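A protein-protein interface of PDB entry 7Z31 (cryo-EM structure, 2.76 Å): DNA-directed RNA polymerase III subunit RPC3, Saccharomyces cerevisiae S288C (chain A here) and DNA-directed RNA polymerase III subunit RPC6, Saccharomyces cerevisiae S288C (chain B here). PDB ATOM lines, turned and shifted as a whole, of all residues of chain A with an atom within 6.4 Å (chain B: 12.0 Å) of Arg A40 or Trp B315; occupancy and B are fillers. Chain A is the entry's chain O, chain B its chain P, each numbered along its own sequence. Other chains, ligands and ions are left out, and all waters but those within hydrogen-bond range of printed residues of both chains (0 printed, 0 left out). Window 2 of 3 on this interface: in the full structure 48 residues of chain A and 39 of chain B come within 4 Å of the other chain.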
ATOM      1  N   SER A  35       9.304  -9.088 -12.563  1.00  0.00           N
ATOM      2  CA  SER A  35       9.961  -9.314 -13.846  1.00  0.00           C
ATOM      3  C   SER A  35      11.160  -8.397 -14.056  1.00  0.00           C
ATOM      4  O   SER A  35      12.159  -8.816 -14.648  1.00  0.00           O
ATOM      5  CB  SER A  35       8.961  -9.114 -14.979  1.00  0.00           C
ATOM      6  OG  SER A  35       8.486  -7.779 -14.982  1.00  0.00           O
ATOM      7  N   SER A  36      11.078  -7.148 -13.596  1.00  0.00           N
ATOM      8  CA  SER A  36      12.139  -6.158 -13.788  1.00  0.00           C
ATOM      9  C   SER A  36      12.420  -5.929 -15.277  1.00  0.00           C
ATOM     10  O   SER A  36      13.494  -6.238 -15.796  1.00  0.00           O
ATOM     11  CB  SER A  36      13.410  -6.564 -13.034  1.00  0.00           C
ATOM     12  OG  SER A  36      14.542  -5.877 -13.536  1.00  0.00           O
ATOM     13  N   LEU A  37      11.410  -5.389 -15.964  1.00  0.00           N
ATOM     14  CA  LEU A  37      11.543  -4.984 -17.359  1.00  0.00           C
ATOM     15  C   LEU A  37      11.914  -3.513 -17.508  1.00  0.00           C
ATOM     16  O   LEU A  37      12.420  -3.114 -18.562  1.00  0.00           O
ATOM     17  CB  LEU A  37      10.236  -5.291 -18.108  1.00  0.00           C
ATOM     18  CG  LEU A  37       9.911  -4.709 -19.487  1.00  0.00           C
ATOM     19  CD1 LEU A  37      10.953  -5.097 -20.523  1.00  0.00           C
ATOM     20  CD2 LEU A  37       8.527  -5.159 -19.933  1.00  0.00           C
ATOM     21  N   GLU A  38      11.700  -2.707 -16.468  1.00  0.00           N
ATOM     22  CA  GLU A  38      12.130  -1.313 -16.508  1.00  0.00           C
ATOM     23  C   GLU A  38      13.646  -1.196 -16.626  1.00  0.00           C
ATOM     24  O   GLU A  38      14.140  -0.361 -17.390  1.00  0.00           O
ATOM     25  CB  GLU A  38      11.618  -0.568 -15.272  1.00  0.00           C
ATOM     26  CG  GLU A  38      12.068  -1.129 -13.925  1.00  0.00           C
ATOM     27  CD  GLU A  38      11.312  -2.381 -13.492  1.00  0.00           C
ATOM     28  OE1 GLU A  38      10.890  -3.174 -14.361  1.00  0.00           O
ATOM     29  OE2 GLU A  38      11.142  -2.572 -12.268  1.00  0.00           O
ATOM     30  N   GLN A  39      14.398  -2.029 -15.895  1.00  0.00           N
ATOM     31  CA  GLN A  39      15.856  -2.008 -15.980  1.00  0.00           C
ATOM     32  C   GLN A  39      16.377  -2.646 -17.254  1.00  0.00           C
ATOM     33  O   GLN A  39      17.519  -2.382 -17.644  1.00  0.00           O
ATOM     34  CB  GLN A  39      16.487  -2.731 -14.787  1.00  0.00           C
ATOM     35  CG  GLN A  39      16.203  -2.115 -13.443  1.00  0.00           C
ATOM     36  CD  GLN A  39      14.896  -2.590 -12.870  1.00  0.00           C
ATOM     37  OE1 GLN A  39      14.290  -3.524 -13.386  1.00  0.00           O
ATOM     38  NE2 GLN A  39      14.442  -1.941 -11.808  1.00  0.00           N
ATOM     39  N   ARG A  40      15.578  -3.493 -17.901  1.00  0.00           N
ATOM     40  CA  ARG A  40      16.038  -4.187 -19.093  1.00  0.00           C
ATOM     41  C   ARG A  40      16.331  -3.225 -20.237  1.00  0.00           C
ATOM     42  O   ARG A  40      17.081  -3.580 -21.151  1.00  0.00           O
ATOM     43  CB  ARG A  40      14.996  -5.222 -19.523  1.00  0.00           C
ATOM     44  CG  ARG A  40      15.571  -6.442 -20.211  1.00  0.00           C
ATOM     45  CD  ARG A  40      14.466  -7.389 -20.657  1.00  0.00           C
ATOM     46  NE  ARG A  40      13.397  -7.497 -19.671  1.00  0.00           N
ATOM     47  CZ  ARG A  40      13.471  -8.218 -18.560  1.00  0.00           C
ATOM     48  NH1 ARG A  40      14.560  -8.899 -18.251  1.00  0.00           N
ATOM     49  NH2 ARG A  40      12.427  -8.252 -17.737  1.00  0.00           N
ATOM     50  N   THR A  41      15.765  -2.022 -20.198  1.00  0.00           N
ATOM     51  CA  THR A  41      15.932  -1.027 -21.247  1.00  0.00           C
ATOM     52  C   THR A  41      17.105  -0.087 -20.995  1.00  0.00           C
ATOM     53  O   THR A  41      17.368   0.790 -21.826  1.00  0.00           O
ATOM     54  CB  THR A  41      14.648  -0.208 -21.404  1.00  0.00           C
ATOM     55  OG1 THR A  41      14.369   0.478 -20.179  1.00  0.00           O
ATOM     56  CG2 THR A  41      13.478  -1.114 -21.753  1.00  0.00           C
ATOM     57  N   LEU A  42      17.798  -0.234 -19.870  1.00  0.00           N
ATOM     58  CA  LEU A  42      19.001   0.540 -19.612  1.00  0.00           C
ATOM     59  C   LEU A  42      20.163  -0.015 -20.422  1.00  0.00           C
ATOM     60  O   LEU A  42      20.215  -1.211 -20.722  1.00  0.00           O
ATOM     61  CB  LEU A  42      19.354   0.504 -18.125  1.00  0.00           C
ATOM     62  CG  LEU A  42      18.385   1.130 -17.128  1.00  0.00           C
ATOM     63  CD1 LEU A  42      18.606   0.530 -15.753  1.00  0.00           C
ATOM     64  CD2 LEU A  42      18.575   2.626 -17.091  1.00  0.00           C
ATOM     65  N   ASN A  43      21.085   0.857 -20.785  1.00  0.00           N
ATOM     66  CA  ASN A  43      22.358   0.394 -21.312  1.00  0.00           C
ATOM     67  C   ASN A  43      23.127  -0.301 -20.195  1.00  0.00           C
ATOM     68  O   ASN A  43      23.226   0.243 -19.089  1.00  0.00           O
ATOM     69  CB  ASN A  43      23.163   1.557 -21.874  1.00  0.00           C
ATOM     70  CG  ASN A  43      22.872   1.820 -23.334  1.00  0.00           C
ATOM     71  OD1 ASN A  43      21.794   1.505 -23.836  1.00  0.00           O
ATOM     72  ND2 ASN A  43      23.842   2.398 -24.029  1.00  0.00           N
ATOM     73  N   PRO A  44      23.665  -1.499 -20.429  1.00  0.00           N
ATOM     74  CA  PRO A  44      24.320  -2.231 -19.333  1.00  0.00           C
ATOM     75  C   PRO A  44      25.504  -1.501 -18.728  1.00  0.00           C
ATOM     76  O   PRO A  44      25.739  -1.619 -17.519  1.00  0.00           O
ATOM     77  CB  PRO A  44      24.754  -3.544 -20.001  1.00  0.00           C
ATOM     78  CG  PRO A  44      23.930  -3.647 -21.238  1.00  0.00           C
ATOM     79  CD  PRO A  44      23.726  -2.243 -21.698  1.00  0.00           C
ATOM     80  N   PHE A  47      24.287   1.052 -16.199  1.00  0.00           N
ATOM     81  CA  PHE A  47      23.613   0.409 -15.075  1.00  0.00           C
ATOM     82  C   PHE A  47      24.614  -0.054 -14.021  1.00  0.00           C
ATOM     83  O   PHE A  47      24.473   0.259 -12.832  1.00  0.00           O
ATOM     84  CB  PHE A  47      22.787  -0.763 -15.607  1.00  0.00           C
ATOM     85  CG  PHE A  47      21.756  -1.286 -14.652  1.00  0.00           C
ATOM     86  CD1 PHE A  47      21.560  -0.704 -13.411  1.00  0.00           C
ATOM     87  CD2 PHE A  47      20.981  -2.377 -15.001  1.00  0.00           C
ATOM     88  CE1 PHE A  47      20.611  -1.202 -12.545  1.00  0.00           C
ATOM     89  CE2 PHE A  47      20.037  -2.875 -14.139  1.00  0.00           C
ATOM     90  CZ  PHE A  47      19.850  -2.287 -12.910  1.00  0.00           C
ATOM     91  N   PHE A 576      28.593  -8.634 -27.829  1.00  0.00           N
ATOM     92  CA  PHE A 576      27.382  -9.086 -27.150  1.00  0.00           C
ATOM     93  C   PHE A 576      27.681  -9.653 -25.766  1.00  0.00           C
ATOM     94  O   PHE A 576      26.989  -9.336 -24.794  1.00  0.00           O
ATOM     95  CB  PHE A 576      26.664 -10.124 -28.010  1.00  0.00           C
ATOM     96  CG  PHE A 576      25.598 -10.889 -27.276  1.00  0.00           C
ATOM     97  CD1 PHE A 576      24.519 -10.233 -26.707  1.00  0.00           C
ATOM     98  CD2 PHE A 576      25.668 -12.268 -27.166  1.00  0.00           C
ATOM     99  CE1 PHE A 576      23.537 -10.936 -26.038  1.00  0.00           C
ATOM    100  CE2 PHE A 576      24.686 -12.974 -26.500  1.00  0.00           C
ATOM    101  CZ  PHE A 576      23.621 -12.307 -25.937  1.00  0.00           C
ATOM    102  N   GLN A 579      28.145  -6.958 -23.024  1.00  0.00           N
ATOM    103  CA  GLN A 579      26.998  -6.211 -22.524  1.00  0.00           C
ATOM    104  C   GLN A 579      26.066  -7.075 -21.684  1.00  0.00           C
ATOM    105  O   GLN A 579      25.561  -6.611 -20.662  1.00  0.00           O
ATOM    106  CB  GLN A 579      26.242  -5.566 -23.685  1.00  0.00           C
ATOM    107  CG  GLN A 579      26.169  -6.423 -24.921  1.00  0.00           C
ATOM    108  CD  GLN A 579      25.817  -5.636 -26.159  1.00  0.00           C
ATOM    109  OE1 GLN A 579      24.850  -4.877 -26.174  1.00  0.00           O
ATOM    110  NE2 GLN A 579      26.614  -5.801 -27.208  1.00  0.00           N
ATOM    111  N   ASN A 580      25.812  -8.323 -22.089  1.00  0.00           N
ATOM    112  CA  ASN A 580      24.942  -9.187 -21.293  1.00  0.00           C
ATOM    113  C   ASN A 580      25.517  -9.405 -19.897  1.00  0.00           C
ATOM    114  O   ASN A 580      24.811  -9.266 -18.890  1.00  0.00           O
ATOM    115  CB  ASN A 580      24.728 -10.523 -22.013  1.00  0.00           C
ATOM    116  CG  ASN A 580      23.792 -11.477 -21.261  1.00  0.00           C
ATOM    117  OD1 ASN A 580      23.825 -11.586 -20.035  1.00  0.00           O
ATOM    118  ND2 ASN A 580      22.966 -12.191 -22.013  1.00  0.00           N
ATOM    119  N   TRP A 583      25.364  -6.293 -17.862  1.00  0.00           N
ATOM    120  CA  TRP A 583      23.986  -6.079 -17.435  1.00  0.00           C
ATOM    121  C   TRP A 583      23.623  -6.974 -16.263  1.00  0.00           C
ATOM    122  O   TRP A 583      22.910  -6.553 -15.350  1.00  0.00           O
ATOM    123  CB  TRP A 583      23.039  -6.333 -18.611  1.00  0.00           C
ATOM    124  CG  TRP A 583      21.591  -6.136 -18.298  1.00  0.00           C
ATOM    125  CD1 TRP A 583      20.895  -4.968 -18.351  1.00  0.00           C
ATOM    126  CD2 TRP A 583      20.654  -7.143 -17.900  1.00  0.00           C
ATOM    127  NE1 TRP A 583      19.585  -5.180 -18.005  1.00  0.00           N
ATOM    128  CE2 TRP A 583      19.412  -6.508 -17.722  1.00  0.00           C
ATOM    129  CE3 TRP A 583      20.745  -8.518 -17.678  1.00  0.00           C
ATOM    130  CZ2 TRP A 583      18.272  -7.200 -17.332  1.00  0.00           C
ATOM    131  CZ3 TRP A 583      19.611  -9.203 -17.289  1.00  0.00           C
ATOM    132  CH2 TRP A 583      18.393  -8.545 -17.123  1.00  0.00           C
ATOM    133  N   ASN A 584      24.084  -8.223 -16.279  1.00  0.00           N
ATOM    134  CA  ASN A 584      23.733  -9.138 -15.198  1.00  0.00           C
ATOM    135  C   ASN A 584      24.414  -8.740 -13.895  1.00  0.00           C
ATOM    136  O   ASN A 584      23.797  -8.792 -12.822  1.00  0.00           O
ATOM    137  CB  ASN A 584      24.081 -10.569 -15.596  1.00  0.00           C
ATOM    138  CG  ASN A 584      23.143 -11.111 -16.648  1.00  0.00           C
ATOM    139  OD1 ASN A 584      22.108 -11.693 -16.325  1.00  0.00           O
ATOM    140  ND2 ASN A 584      23.488 -10.909 -17.914  1.00  0.00           N
ATOM    141  N   ASN A 587      22.442  -5.919 -12.630  1.00  0.00           N
ATOM    142  CA  ASN A 587      21.232  -6.408 -11.983  1.00  0.00           C
ATOM    143  C   ASN A 587      21.527  -6.912 -10.577  1.00  0.00           C
ATOM    144  O   ASN A 587      20.747  -6.681  -9.650  1.00  0.00           O
ATOM    145  CB  ASN A 587      20.604  -7.518 -12.823  1.00  0.00           C
ATOM    146  CG  ASN A 587      19.405  -7.046 -13.607  1.00  0.00           C
ATOM    147  OD1 ASN A 587      19.206  -5.847 -13.801  1.00  0.00           O
ATOM    148  ND2 ASN A 587      18.593  -7.988 -14.065  1.00  0.00           N
ATOM    149  N   VAL B 309      18.845 -15.291  -8.796  1.00  0.00           N
ATOM    150  CA  VAL B 309      19.334 -16.248  -9.781  1.00  0.00           C
ATOM    151  C   VAL B 309      19.619 -15.519 -11.085  1.00  0.00           C
ATOM    152  O   VAL B 309      18.792 -14.737 -11.567  1.00  0.00           O
ATOM    153  CB  VAL B 309      18.315 -17.381  -9.993  1.00  0.00           C
ATOM    154  CG1 VAL B 309      18.718 -18.239 -11.179  1.00  0.00           C
ATOM    155  CG2 VAL B 309      18.193 -18.226  -8.736  1.00  0.00           C
ATOM    156  N   VAL B 310      20.785 -15.774 -11.657  1.00  0.00           N
ATOM    157  CA  VAL B 310      21.209 -15.160 -12.909  1.00  0.00           C
ATOM    158  C   VAL B 310      20.773 -16.037 -14.076  1.00  0.00           C
ATOM    159  O   VAL B 310      20.736 -17.267 -13.981  1.00  0.00           O
ATOM    160  CB  VAL B 310      22.736 -14.934 -12.906  1.00  0.00           C
ATOM    161  CG1 VAL B 310      23.177 -14.177 -14.145  1.00  0.00           C
ATOM    162  CG2 VAL B 310      23.154 -14.206 -11.637  1.00  0.00           C
ATOM    163  N   TYR B 311      20.424 -15.391 -15.187  1.00  0.00           N
ATOM    164  CA  TYR B 311      20.062 -16.063 -16.426  1.00  0.00           C
ATOM    165  C   TYR B 311      20.801 -15.394 -17.577  1.00  0.00           C
ATOM    166  O   TYR B 311      21.253 -14.251 -17.468  1.00  0.00           O
ATOM    167  CB  TYR B 311      18.549 -16.025 -16.670  1.00  0.00           C
ATOM    168  CG  TYR B 311      17.730 -16.393 -15.454  1.00  0.00           C
ATOM    169  CD1 TYR B 311      17.345 -15.427 -14.539  1.00  0.00           C
ATOM    170  CD2 TYR B 311      17.344 -17.707 -15.222  1.00  0.00           C
ATOM    171  CE1 TYR B 311      16.598 -15.755 -13.424  1.00  0.00           C
ATOM    172  CE2 TYR B 311      16.597 -18.046 -14.110  1.00  0.00           C
ATOM    173  CZ  TYR B 311      16.227 -17.065 -13.213  1.00  0.00           C
ATOM    174  OH  TYR B 311      15.487 -17.389 -12.102  1.00  0.00           O
ATOM    175  N   PHE B 312      20.928 -16.122 -18.685  1.00  0.00           N
ATOM    176  CA  PHE B 312      21.673 -15.620 -19.834  1.00  0.00           C
ATOM    177  C   PHE B 312      20.774 -15.056 -20.924  1.00  0.00           C
ATOM    178  O   PHE B 312      21.153 -14.083 -21.585  1.00  0.00           O
ATOM    179  CB  PHE B 312      22.555 -16.731 -20.413  1.00  0.00           C
ATOM    180  CG  PHE B 312      23.166 -16.396 -21.738  1.00  0.00           C
ATOM    181  CD1 PHE B 312      23.989 -15.295 -21.881  1.00  0.00           C
ATOM    182  CD2 PHE B 312      22.925 -17.192 -22.841  1.00  0.00           C
ATOM    183  CE1 PHE B 312      24.551 -14.992 -23.101  1.00  0.00           C
ATOM    184  CE2 PHE B 312      23.489 -16.896 -24.061  1.00  0.00           C
ATOM    185  CZ  PHE B 312      24.301 -15.791 -24.194  1.00  0.00           C
ATOM    186  N   ASP B 313      19.602 -15.643 -21.134  1.00  0.00           N
ATOM    187  CA  ASP B 313      18.634 -15.126 -22.094  1.00  0.00           C
ATOM    188  C   ASP B 313      17.797 -13.989 -21.527  1.00  0.00           C
ATOM    189  O   ASP B 313      17.077 -13.331 -22.288  1.00  0.00           O
ATOM    190  CB  ASP B 313      17.709 -16.257 -22.568  1.00  0.00           C
ATOM    191  CG  ASP B 313      17.012 -16.965 -21.414  1.00  0.00           C
ATOM    192  OD1 ASP B 313      17.220 -16.569 -20.246  1.00  0.00           O
ATOM    193  OD2 ASP B 313      16.259 -17.926 -21.676  1.00  0.00           O
ATOM    194  N   GLU B 314      17.880 -13.749 -20.215  1.00  0.00           N
ATOM    195  CA  GLU B 314      16.986 -12.803 -19.549  1.00  0.00           C
ATOM    196  C   GLU B 314      17.115 -11.403 -20.129  1.00  0.00           C
ATOM    197  O   GLU B 314      16.126 -10.668 -20.222  1.00  0.00           O
ATOM    198  CB  GLU B 314      17.282 -12.786 -18.048  1.00  0.00           C
ATOM    199  CG  GLU B 314      16.331 -11.949 -17.224  1.00  0.00           C
ATOM    200  CD  GLU B 314      14.908 -12.453 -17.306  1.00  0.00           C
ATOM    201  OE1 GLU B 314      14.712 -13.667 -17.542  1.00  0.00           O
ATOM    202  OE2 GLU B 314      13.981 -11.636 -17.141  1.00  0.00           O
ATOM    203  N   TRP B 315      18.330 -11.015 -20.517  1.00  0.00           N
ATOM    204  CA  TRP B 315      18.548  -9.683 -21.070  1.00  0.00           C
ATOM    205  C   TRP B 315      17.742  -9.476 -22.345  1.00  0.00           C
ATOM    206  O   TRP B 315      17.121  -8.423 -22.533  1.00  0.00           O
ATOM    207  CB  TRP B 315      20.037  -9.482 -21.333  1.00  0.00           C
ATOM    208  CG  TRP B 315      20.420  -8.093 -21.698  1.00  0.00           C
ATOM    209  CD1 TRP B 315      20.107  -6.955 -21.021  1.00  0.00           C
ATOM    210  CD2 TRP B 315      21.225  -7.693 -22.809  1.00  0.00           C
ATOM    211  NE1 TRP B 315      20.656  -5.864 -21.650  1.00  0.00           N
ATOM    212  CE2 TRP B 315      21.345  -6.291 -22.753  1.00  0.00           C
ATOM    213  CE3 TRP B 315      21.848  -8.383 -23.851  1.00  0.00           C
ATOM    214  CZ2 TRP B 315      22.066  -5.570 -23.694  1.00  0.00           C
ATOM    215  CZ3 TRP B 315      22.559  -7.665 -24.783  1.00  0.00           C
ATOM    216  CH2 TRP B 315      22.660  -6.271 -24.700  1.00  0.00           C
ATOM    217  N   THR B 316      17.735 -10.465 -23.229  1.00  0.00           N
ATOM    218  CA  THR B 316      16.946 -10.375 -24.451  1.00  0.00           C
ATOM    219  C   THR B 316      15.699 -11.250 -24.340  1.00  0.00           C
ATOM    220  O   THR B 316      14.575 -10.759 -24.421  1.00  0.00           O
ATOM    221  CB  THR B 316      17.765 -10.792 -25.690  1.00  0.00           C
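Of the 8 printed residues of chain B, 5 touch a printed residue of chain A. Hydrophobic or aromatic side chains of chain B that line the printed part of chain A: Val B310, Phe B312 and Trp B315. Of the 17 printed residues of chain A, 7 touch a printed residue of chain B. Printed residues of chain A that touch a printed residue of chain B: Arg A40, Pro A44, Phe A576, Gln A579, Asn A580, Trp A583 and Asn A584. Hydrophobic or aromatic side chains of chain A that line the printed part of chain B: Pro A44, Phe A576 and Trp A583. Among the printed residues, 11 pairs touch across the chains. Among the printed residues, Asp or Glu carboxylates within 4 Å of a Lys or Arg side-chain nitrogen of the other chain: Arg A40 with Glu B314 (3.0 Å).
NH1 of Arg A40 lies within salt-bridge range of OE2 of Glu B314. ND2 of Asn A580 is in hydrogen-bond range of O of Phe B312. OD1 of Asn A584 lies close to O of Tyr B311 (2.9 Å).
Of chain B, only Glu B314 and Trp B315 come within 4 Å of Arg A40. Printed residues of chain A within 4 Å of Trp B315: Arg A40, Pro A44, Phe A576, Gln A579 and Trp A583. No residue of chain B comes within 4 Å of Ser A35. Ser A36 touches none of the printed residues of chain B. No residue of chain B comes within 4 Å of Glu A38. No residue of chain B comes within 4 Å of Gln A39. No residue of chain B comes within 4 Å of Leu A42. Of the printed residues of chain A, Glu B314 touches Arg A40 and Trp A583. Of the printed residues of chain B, Trp A583 touches Glu B314 and Trp B315. Of the printed residues of chain A, Val B310 touches Asn A584. Printed residues of chain B within 4 Å of Asn A584: Val B310 and Tyr B311. The nearest residue of chain B that does not touch Arg A40 is Thr B316 (5.1 Å).
O of Ser A35 sits at hydrogen-bond distance from NH2 of Arg A40, at 3.2 Å. NH2 of Arg A40 is in hydrogen-bond range of O of Ser A36 (3.0 Å). The backbone carbonyl oxygen (O) of Gln A39 lies within hydrogen-bond range of the indole nitrogen (NE1) of Trp A583, at 3.5 Å.
Among the printed residues, merely in contact across the chains: Gln A579 with Trp B315, Trp A583 with Trp B315, Arg A40 with Trp B315, Asn A584 with Val B310, Pro A44 with Trp B315, Phe A576 with Trp B315, Phe A576 with Phe B312 and Trp A583 with Glu B314.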
